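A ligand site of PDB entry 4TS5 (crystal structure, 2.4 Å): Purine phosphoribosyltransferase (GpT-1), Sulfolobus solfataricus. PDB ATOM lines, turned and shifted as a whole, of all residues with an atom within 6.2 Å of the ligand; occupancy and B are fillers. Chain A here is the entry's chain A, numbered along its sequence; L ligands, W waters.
OD2 of Asp 96 sits at hydrogen-bond distance from O7 of the ligand, 2.8 Å away. O3 of the ligand is in hydrogen-bond range of OG1 of Thr 100. N of Ser 103 is in hydrogen-bond range of O2 of the ligand, at 3.0 Å. An oxygen (O1) of the ligand lies within hydrogen-bond range of the backbone NH (N) of Thr 100 (3.1 Å). N of Phe 149 lies within hydrogen-bond range of N4 of the ligand (2.9 Å). The side-chain hydroxyl (OG) of Ser 103 is in hydrogen-bond range of an oxygen (O2) of the ligand, 2.8 Å away. N of Gly 101 lies within hydrogen-bond range of O1 of the ligand, at 2.8 Å. O6 of the ligand is in hydrogen-bond range of OD2 of Asp 95 (3.2 Å). A nitrogen (N3) of the ligand sits at hydrogen-bond distance from the backbone carbonyl oxygen (O) of Ala 147 (2.8 Å). The backbone NH of Asp 99 is in hydrogen-bond range of an oxygen (O1) of the ligand. A nitrogen (N2) of the ligand is in hydrogen-bond range of the side-chain carboxylate of Asp 99 (2.6 Å).
OD1 of Asp 95 lies within hydrogen-bond range of N of Gly 42, at 3.3 Å. OG of Ser 103 is in hydrogen-bond range of NE2 of His 65, at 2.7 Å. The side-chain hydroxyl (OG1) of Thr 100 is in hydrogen-bond range of the backbone NH (N) of Asp 102 (3.1 Å). The indole nitrogen (NE1) of Trp 148 lies within hydrogen-bond range of the side-chain carboxylate (OD2) of Asp 158, at 2.9 Å. OD1 of Asp 99 is in hydrogen-bond range of NE1 of Trp 146 (3.0 Å). N of Ile 128 sits at hydrogen-bond distance from O of Thr 98, 3.0 Å away.
His 65 touches the ligand (NE2 to C1, 3.5 Å). CG2 of Ile 97 touches C4 of the ligand (3.6 Å). Thr 98 touches the ligand. N of Asp 102 touches O2 of the ligand (3.6 Å). CD1 of Ile 128 touches N3 of the ligand, 3.7 Å away. Trp 146 touches the ligand (NE1 to N3, 3.7 Å). Trp 148 touches the ligand (CH2 to N5, 3.3 Å). Hydrophobic or aromatic side chains within 4 Å of the ligand: His 65, Ile 97, Ile 128, Trp 146, Trp 148 and Phe 149. The nearest printed residue that does not touch the ligand is Tyr 151 (4.002 Å).
Water W2 lies within hydrogen-bond range of an oxygen (O1) of the ligand (2.8 Å), the backbone NH of Ile 104 (3.0 Å) and the backbone NH of Ser 103 (3.4 Å). Water W3 lies within hydrogen-bond range of the side-chain carboxylate of Asp 95 (2.8 Å), an oxygen (O6) of the ligand (2.9 Å), the side-chain hydroxyl of Ser 103 (3.1 Å) and a ring nitrogen (NE2) of His 65 (3.2 Å).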
ATOM      1  N   ILE A  38      -6.596  21.504 -14.886  1.00  0.00           N
ATOM      2  CA  ILE A  38      -7.589  21.868 -13.895  1.00  0.00           C
ATOM      3  C   ILE A  38      -6.896  22.379 -12.624  1.00  0.00           C
ATOM      4  O   ILE A  38      -6.180  21.619 -11.955  1.00  0.00           O
ATOM      5  CB  ILE A  38      -8.512  20.663 -13.561  1.00  0.00           C
ATOM      6  CG1 ILE A  38      -9.324  20.266 -14.814  1.00  0.00           C
ATOM      7  CG2 ILE A  38      -9.432  21.001 -12.426  1.00  0.00           C
ATOM      8  CD1 ILE A  38     -10.104  18.982 -14.647  1.00  0.00           C
ATOM      9  N   GLY A  41      -5.349  21.240  -8.603  1.00  0.00           N
ATOM     10  CA  GLY A  41      -4.774  19.899  -8.490  1.00  0.00           C
ATOM     11  C   GLY A  41      -4.016  19.427  -9.718  1.00  0.00           C
ATOM     12  O   GLY A  41      -3.119  18.604  -9.609  1.00  0.00           O
ATOM     13  N   GLY A  42      -4.376  19.944 -10.890  1.00  0.00           N
ATOM     14  CA  GLY A  42      -3.781  19.467 -12.121  1.00  0.00           C
ATOM     15  C   GLY A  42      -2.603  20.289 -12.602  1.00  0.00           C
ATOM     16  O   GLY A  42      -1.981  19.936 -13.608  1.00  0.00           O
ATOM     17  N   HIS A  65     -15.172  23.134  -5.764  1.00  0.00           N
ATOM     18  CA  HIS A  65     -15.979  21.991  -5.324  1.00  0.00           C
ATOM     19  C   HIS A  65     -16.870  22.400  -4.160  1.00  0.00           C
ATOM     20  O   HIS A  65     -16.400  22.632  -3.031  1.00  0.00           O
ATOM     21  CB  HIS A  65     -15.070  20.813  -4.964  1.00  0.00           C
ATOM     22  CG  HIS A  65     -14.119  20.457  -6.059  1.00  0.00           C
ATOM     23  ND1 HIS A  65     -12.860  21.001  -6.160  1.00  0.00           N
ATOM     24  CD2 HIS A  65     -14.261  19.653  -7.137  1.00  0.00           C
ATOM     25  CE1 HIS A  65     -12.262  20.536  -7.238  1.00  0.00           C
ATOM     26  NE2 HIS A  65     -13.097  19.715  -7.850  1.00  0.00           N
ATOM     27  N   ALA A  76     -19.430  20.818  -8.760  1.00  0.00           N
ATOM     28  CA  ALA A  76     -18.194  21.391  -9.257  1.00  0.00           C
ATOM     29  C   ALA A  76     -18.554  22.633 -10.058  1.00  0.00           C
ATOM     30  O   ALA A  76     -19.614  22.694 -10.683  1.00  0.00           O
ATOM     31  CB  ALA A  76     -17.460  20.382 -10.118  1.00  0.00           C
ATOM     32  N   ASP A  95      -5.875  16.439 -14.662  1.00  0.00           N
ATOM     33  CA  ASP A  95      -6.072  16.653 -13.222  1.00  0.00           C
ATOM     34  C   ASP A  95      -5.238  15.625 -12.468  1.00  0.00           C
ATOM     35  O   ASP A  95      -4.695  14.689 -13.059  1.00  0.00           O
ATOM     36  CB  ASP A  95      -7.554  16.523 -12.840  1.00  0.00           C
ATOM     37  CG  ASP A  95      -7.947  17.441 -11.692  1.00  0.00           C
ATOM     38  OD1 ASP A  95      -7.051  18.051 -11.054  1.00  0.00           O
ATOM     39  OD2 ASP A  95      -9.157  17.568 -11.422  1.00  0.00           O
ATOM     40  N   ASP A  96      -5.151  15.800 -11.142  1.00  0.00           N
ATOM     41  CA  ASP A  96      -4.364  14.903 -10.317  1.00  0.00           C
ATOM     42  C   ASP A  96      -4.994  13.523 -10.187  1.00  0.00           C
ATOM     43  O   ASP A  96      -4.346  12.515 -10.459  1.00  0.00           O
ATOM     44  CB  ASP A  96      -4.103  15.517  -8.933  1.00  0.00           C
ATOM     45  CG  ASP A  96      -5.332  16.146  -8.318  1.00  0.00           C
ATOM     46  OD1 ASP A  96      -6.462  15.898  -8.817  1.00  0.00           O
ATOM     47  OD2 ASP A  96      -5.175  16.893  -7.334  1.00  0.00           O
ATOM     48  N   ILE A  97      -6.268  13.479  -9.787  1.00  0.00           N
ATOM     49  CA  ILE A  97      -6.951  12.207  -9.542  1.00  0.00           C
ATOM     50  C   ILE A  97      -8.432  12.266  -9.868  1.00  0.00           C
ATOM     51  O   ILE A  97      -9.103  13.246  -9.569  1.00  0.00           O
ATOM     52  CB  ILE A  97      -6.761  11.752  -8.082  1.00  0.00           C
ATOM     53  CG1 ILE A  97      -7.447  10.410  -7.828  1.00  0.00           C
ATOM     54  CG2 ILE A  97      -7.269  12.815  -7.103  1.00  0.00           C
ATOM     55  CD1 ILE A  97      -7.179   9.837  -6.426  1.00  0.00           C
ATOM     56  N   THR A  98      -8.941  11.230 -10.520  1.00  0.00           N
ATOM     57  CA  THR A  98     -10.363  11.088 -10.702  1.00  0.00           C
ATOM     58  C   THR A  98     -10.937  10.295  -9.527  1.00  0.00           C
ATOM     59  O   THR A  98     -10.602   9.122  -9.318  1.00  0.00           O
ATOM     60  CB  THR A  98     -10.708  10.339 -11.997  1.00  0.00           C
ATOM     61  OG1 THR A  98     -10.289  11.128 -13.118  1.00  0.00           O
ATOM     62  CG2 THR A  98     -12.204  10.098 -12.071  1.00  0.00           C
ATOM     63  N   ASP A  99     -11.772  10.959  -8.734  1.00  0.00           N
ATOM     64  CA  ASP A  99     -12.449  10.289  -7.636  1.00  0.00           C
ATOM     65  C   ASP A  99     -13.869   9.910  -8.064  1.00  0.00           C
ATOM     66  O   ASP A  99     -14.118   8.772  -8.479  1.00  0.00           O
ATOM     67  CB  ASP A  99     -12.459  11.172  -6.381  1.00  0.00           C
ATOM     68  CG  ASP A  99     -12.784  10.397  -5.115  1.00  0.00           C
ATOM     69  OD1 ASP A  99     -12.257  10.752  -4.051  1.00  0.00           O
ATOM     70  OD2 ASP A  99     -13.547   9.412  -5.178  1.00  0.00           O
ATOM     71  N   THR A 100     -14.781  10.870  -7.969  1.00  0.00           N
ATOM     72  CA  THR A 100     -16.142  10.680  -8.461  1.00  0.00           C
ATOM     73  C   THR A 100     -16.188  10.901  -9.964  1.00  0.00           C
ATOM     74  O   THR A 100     -17.047  10.368 -10.636  1.00  0.00           O
ATOM     75  CB  THR A 100     -17.151  11.646  -7.799  1.00  0.00           C
ATOM     76  OG1 THR A 100     -16.845  12.991  -8.177  1.00  0.00           O
ATOM     77  CG2 THR A 100     -17.121  11.520  -6.285  1.00  0.00           C
ATOM     78  N   GLY A 101     -15.256  11.699 -10.482  1.00  0.00           N
ATOM     79  CA  GLY A 101     -15.286  12.078 -11.890  1.00  0.00           C
ATOM     80  C   GLY A 101     -16.076  13.359 -12.191  1.00  0.00           C
ATOM     81  O   GLY A 101     -16.154  13.780 -13.335  1.00  0.00           O
ATOM     82  N   ASP A 102     -16.648  13.969 -11.159  1.00  0.00           N
ATOM     83  CA  ASP A 102     -17.376  15.225 -11.305  1.00  0.00           C
ATOM     84  C   ASP A 102     -16.515  16.341 -11.931  1.00  0.00           C
ATOM     85  O   ASP A 102     -16.956  17.050 -12.836  1.00  0.00           O
ATOM     86  CB  ASP A 102     -17.966  15.687  -9.966  1.00  0.00           C
ATOM     87  CG  ASP A 102     -19.159  14.817  -9.501  1.00  0.00           C
ATOM     88  OD1 ASP A 102     -19.560  13.871 -10.215  1.00  0.00           O
ATOM     89  OD2 ASP A 102     -19.683  15.070  -8.385  1.00  0.00           O
ATOM     90  N   SER A 103     -15.284  16.506 -11.460  1.00  0.00           N
ATOM     91  CA  SER A 103     -14.403  17.535 -12.004  1.00  0.00           C
ATOM     92  C   SER A 103     -14.078  17.359 -13.485  1.00  0.00           C
ATOM     93  O   SER A 103     -14.206  18.303 -14.267  1.00  0.00           O
ATOM     94  CB  SER A 103     -13.124  17.647 -11.190  1.00  0.00           C
ATOM     95  OG  SER A 103     -13.434  17.903  -9.836  1.00  0.00           O
ATOM     96  N   ILE A 104     -13.639  16.160 -13.885  1.00  0.00           N
ATOM     97  CA  ILE A 104     -13.277  15.969 -15.289  1.00  0.00           C
ATOM     98  C   ILE A 104     -14.490  16.046 -16.201  1.00  0.00           C
ATOM     99  O   ILE A 104     -14.399  16.523 -17.325  1.00  0.00           O
ATOM    100  CB  ILE A 104     -12.475  14.675 -15.571  1.00  0.00           C
ATOM    101  CG1 ILE A 104     -13.240  13.449 -15.077  1.00  0.00           C
ATOM    102  CG2 ILE A 104     -11.087  14.758 -14.948  1.00  0.00           C
ATOM    103  CD1 ILE A 104     -12.570  12.161 -15.433  1.00  0.00           C
ATOM    104  N   ILE A 128      -9.856   6.218  -9.186  1.00  0.00           N
ATOM    105  CA  ILE A 128     -10.408   5.330  -8.159  1.00  0.00           C
ATOM    106  C   ILE A 128     -11.583   4.543  -8.725  1.00  0.00           C
ATOM    107  O   ILE A 128     -12.688   5.067  -8.848  1.00  0.00           O
ATOM    108  CB  ILE A 128     -10.842   6.105  -6.909  1.00  0.00           C
ATOM    109  CG1 ILE A 128      -9.658   6.913  -6.365  1.00  0.00           C
ATOM    110  CG2 ILE A 128     -11.380   5.149  -5.847  1.00  0.00           C
ATOM    111  CD1 ILE A 128     -10.010   7.840  -5.207  1.00  0.00           C
ATOM    112  N   TRP A 146     -10.453   3.091  -1.946  1.00  0.00           N
ATOM    113  CA  TRP A 146     -10.379   4.528  -1.653  1.00  0.00           C
ATOM    114  C   TRP A 146      -9.379   4.862  -0.552  1.00  0.00           C
ATOM    115  O   TRP A 146      -9.309   4.158   0.458  1.00  0.00           O
ATOM    116  CB  TRP A 146     -11.756   5.083  -1.268  1.00  0.00           C
ATOM    117  CG  TRP A 146     -11.799   6.592  -1.216  1.00  0.00           C
ATOM    118  CD1 TRP A 146     -12.231   7.424  -2.203  1.00  0.00           C
ATOM    119  CD2 TRP A 146     -11.376   7.428  -0.125  1.00  0.00           C
ATOM    120  NE1 TRP A 146     -12.111   8.728  -1.801  1.00  0.00           N
ATOM    121  CE2 TRP A 146     -11.591   8.763  -0.527  1.00  0.00           C
ATOM    122  CE3 TRP A 146     -10.837   7.180   1.142  1.00  0.00           C
ATOM    123  CZ2 TRP A 146     -11.308   9.847   0.296  1.00  0.00           C
ATOM    124  CZ3 TRP A 146     -10.545   8.263   1.956  1.00  0.00           C
ATOM    125  CH2 TRP A 146     -10.787   9.573   1.536  1.00  0.00           C
ATOM    126  N   ALA A 147      -8.585   5.907  -0.772  1.00  0.00           N
ATOM    127  CA  ALA A 147      -7.696   6.438   0.244  1.00  0.00           C
ATOM    128  C   ALA A 147      -7.503   7.898  -0.079  1.00  0.00           C
ATOM    129  O   ALA A 147      -7.718   8.316  -1.212  1.00  0.00           O
ATOM    130  CB  ALA A 147      -6.368   5.701   0.234  1.00  0.00           C
ATOM    131  N   TRP A 148      -7.121   8.702   0.910  1.00  0.00           N
ATOM    132  CA  TRP A 148      -6.804  10.085   0.634  1.00  0.00           C
ATOM    133  C   TRP A 148      -5.349  10.200   0.195  1.00  0.00           C
ATOM    134  O   TRP A 148      -4.446   9.815   0.948  1.00  0.00           O
ATOM    135  CB  TRP A 148      -7.040  11.009   1.831  1.00  0.00           C
ATOM    136  CG  TRP A 148      -6.745  12.430   1.491  1.00  0.00           C
ATOM    137  CD1 TRP A 148      -5.626  13.144   1.819  1.00  0.00           C
ATOM    138  CD2 TRP A 148      -7.564  13.303   0.694  1.00  0.00           C
ATOM    139  NE1 TRP A 148      -5.707  14.419   1.292  1.00  0.00           N
ATOM    140  CE2 TRP A 148      -6.882  14.538   0.600  1.00  0.00           C
ATOM    141  CE3 TRP A 148      -8.811  13.165   0.064  1.00  0.00           C
ATOM    142  CZ2 TRP A 148      -7.409  15.634  -0.096  1.00  0.00           C
ATOM    143  CZ3 TRP A 148      -9.334  14.249  -0.637  1.00  0.00           C
ATOM    144  CH2 TRP A 148      -8.637  15.465  -0.716  1.00  0.00           C
ATOM    145  N   PHE A 149      -5.129  10.720  -1.002  1.00  0.00           N
ATOM    146  CA  PHE A 149      -3.772  10.879  -1.501  1.00  0.00           C
ATOM    147  C   PHE A 149      -3.240  12.258  -1.225  1.00  0.00           C
ATOM    148  O   PHE A 149      -3.729  13.261  -1.760  1.00  0.00           O
ATOM    149  CB  PHE A 149      -3.704  10.521  -2.988  1.00  0.00           C
ATOM    150  CG  PHE A 149      -3.969   9.079  -3.233  1.00  0.00           C
ATOM    151  CD1 PHE A 149      -5.256   8.626  -3.474  1.00  0.00           C
ATOM    152  CD2 PHE A 149      -2.943   8.141  -3.152  1.00  0.00           C
ATOM    153  CE1 PHE A 149      -5.509   7.283  -3.678  1.00  0.00           C
ATOM    154  CE2 PHE A 149      -3.195   6.798  -3.355  1.00  0.00           C
ATOM    155  CZ  PHE A 149      -4.469   6.374  -3.614  1.00  0.00           C
ATOM    156  N   MET A 150      -2.233  12.298  -0.364  1.00  0.00           N
ATOM    157  CA  MET A 150      -1.599  13.540   0.037  1.00  0.00           C
ATOM    158  C   MET A 150      -0.425  13.865  -0.903  1.00  0.00           C
ATOM    159  O   MET A 150       0.668  13.317  -0.771  1.00  0.00           O
ATOM    160  CB  MET A 150      -1.150  13.423   1.483  1.00  0.00           C
ATOM    161  CG  MET A 150      -0.643  14.694   2.118  1.00  0.00           C
ATOM    162  SD  MET A 150      -0.429  14.403   3.893  1.00  0.00           S
ATOM    163  CE  MET A 150       1.109  15.273   4.170  1.00  0.00           C
ATOM    164  N   TYR A 151      -0.674  14.755  -1.867  1.00  0.00           N
ATOM    165  CA  TYR A 151       0.346  15.122  -2.853  1.00  0.00           C
ATOM    166  C   TYR A 151       1.371  16.127  -2.323  1.00  0.00           C
ATOM    167  O   TYR A 151       1.059  16.940  -1.454  1.00  0.00           O
ATOM    168  CB  TYR A 151      -0.330  15.668  -4.125  1.00  0.00           C
ATOM    169  CG  TYR A 151      -1.320  14.681  -4.720  1.00  0.00           C
ATOM    170  CD1 TYR A 151      -2.686  14.947  -4.742  1.00  0.00           C
ATOM    171  CD2 TYR A 151      -0.882  13.470  -5.252  1.00  0.00           C
ATOM    172  CE1 TYR A 151      -3.576  14.048  -5.278  1.00  0.00           C
ATOM    173  CE2 TYR A 151      -1.764  12.561  -5.780  1.00  0.00           C
ATOM    174  CZ  TYR A 151      -3.097  12.845  -5.799  1.00  0.00           C
ATOM    175  OH  TYR A 151      -3.976  11.924  -6.333  1.00  0.00           O
ATOM    176  N   ASN A 154       0.588  19.645  -1.817  1.00  0.00           N
ATOM    177  CA  ASN A 154      -0.555  19.797  -0.935  1.00  0.00           C
ATOM    178  C   ASN A 154      -0.219  19.547   0.539  1.00  0.00           C
ATOM    179  O   ASN A 154      -1.122  19.480   1.368  1.00  0.00           O
ATOM    180  CB  ASN A 154      -1.613  18.767  -1.347  1.00  0.00           C
ATOM    181  CG  ASN A 154      -2.905  19.397  -1.784  1.00  0.00           C
ATOM    182  OD1 ASN A 154      -3.239  19.372  -2.979  1.00  0.00           O
ATOM    183  ND2 ASN A 154      -3.648  19.962  -0.834  1.00  0.00           N
ATOM    184  N   ASP A 158      -3.159  19.795   3.345  1.00  0.00           N
ATOM    185  CA  ASP A 158      -3.707  18.533   3.808  1.00  0.00           C
ATOM    186  C   ASP A 158      -3.451  18.325   5.292  1.00  0.00           C
ATOM    187  O   ASP A 158      -4.343  17.914   6.025  1.00  0.00           O
ATOM    188  CB  ASP A 158      -3.162  17.350   3.011  1.00  0.00           C
ATOM    189  CG  ASP A 158      -3.824  17.220   1.645  1.00  0.00           C
ATOM    190  OD1 ASP A 158      -4.698  18.049   1.328  1.00  0.00           O
ATOM    191  OD2 ASP A 158      -3.470  16.286   0.892  1.00  0.00           O
HETATM  192  P1  LIG L   1     -13.649  14.342  -8.188  1.00  0.00           P
HETATM  193  O1  LIG L   1     -13.304  13.281  -9.202  1.00  0.00           O
HETATM  194  O2  LIG L   1     -14.409  15.510  -8.769  1.00  0.00           O
HETATM  195  O3  LIG L   1     -14.266  13.790  -6.931  1.00  0.00           O
HETATM  196  O4  LIG L   1     -12.214  14.956  -7.729  1.00  0.00           O
HETATM  197  C1  LIG L   1     -12.120  16.336  -7.405  1.00  0.00           C
HETATM  198  C2  LIG L   1     -10.814  16.792  -6.751  1.00  0.00           C
HETATM  199  O5  LIG L   1     -10.793  16.444  -5.363  1.00  0.00           O
HETATM  200  C3  LIG L   1      -9.532  16.242  -7.375  1.00  0.00           C
HETATM  201  O6  LIG L   1      -8.988  17.178  -8.299  1.00  0.00           O
HETATM  202  C4  LIG L   1      -8.576  16.070  -6.199  1.00  0.00           C
HETATM  203  O7  LIG L   1      -7.701  17.198  -6.115  1.00  0.00           O
HETATM  204  C5  LIG L   1      -9.459  16.052  -4.968  1.00  0.00           C
HETATM  205  N1  LIG L   1      -9.580  14.652  -4.513  1.00  0.00           N
HETATM  206  C6  LIG L   1     -10.699  13.910  -4.640  1.00  0.00           C
HETATM  207  N2  LIG L   1     -10.516  12.681  -4.119  1.00  0.00           N
HETATM  208  C7  LIG L   1      -9.267  12.623  -3.646  1.00  0.00           C
HETATM  209  C8  LIG L   1      -8.437  11.608  -2.977  1.00  0.00           C
HETATM  210  N3  LIG L   1      -8.926  10.374  -2.706  1.00  0.00           N
HETATM  211  N4  LIG L   1      -7.172  11.955  -2.645  1.00  0.00           N
HETATM  212  C9  LIG L   1      -6.672  13.183  -2.894  1.00  0.00           C
HETATM  213  N5  LIG L   1      -7.376  14.164  -3.505  1.00  0.00           N
HETATM  214  C10 LIG L   1      -8.651  13.941  -3.900  1.00  0.00           C
HETATM  215  O   HOH W   1     -15.946  16.846  -6.784  1.00  0.00           O
HETATM  216  O   HOH W   2     -12.727  14.306 -11.707  1.00  0.00           O
HETATM  217  O   HOH W   3     -10.571  19.186  -9.660  1.00  0.00           O
HETATM  218  O   HOH W   4      -5.993  16.624  -3.413  1.00  0.00           O
HETATM  219  O   HOH W   5     -14.052  14.241  -4.311  1.00  0.00           O
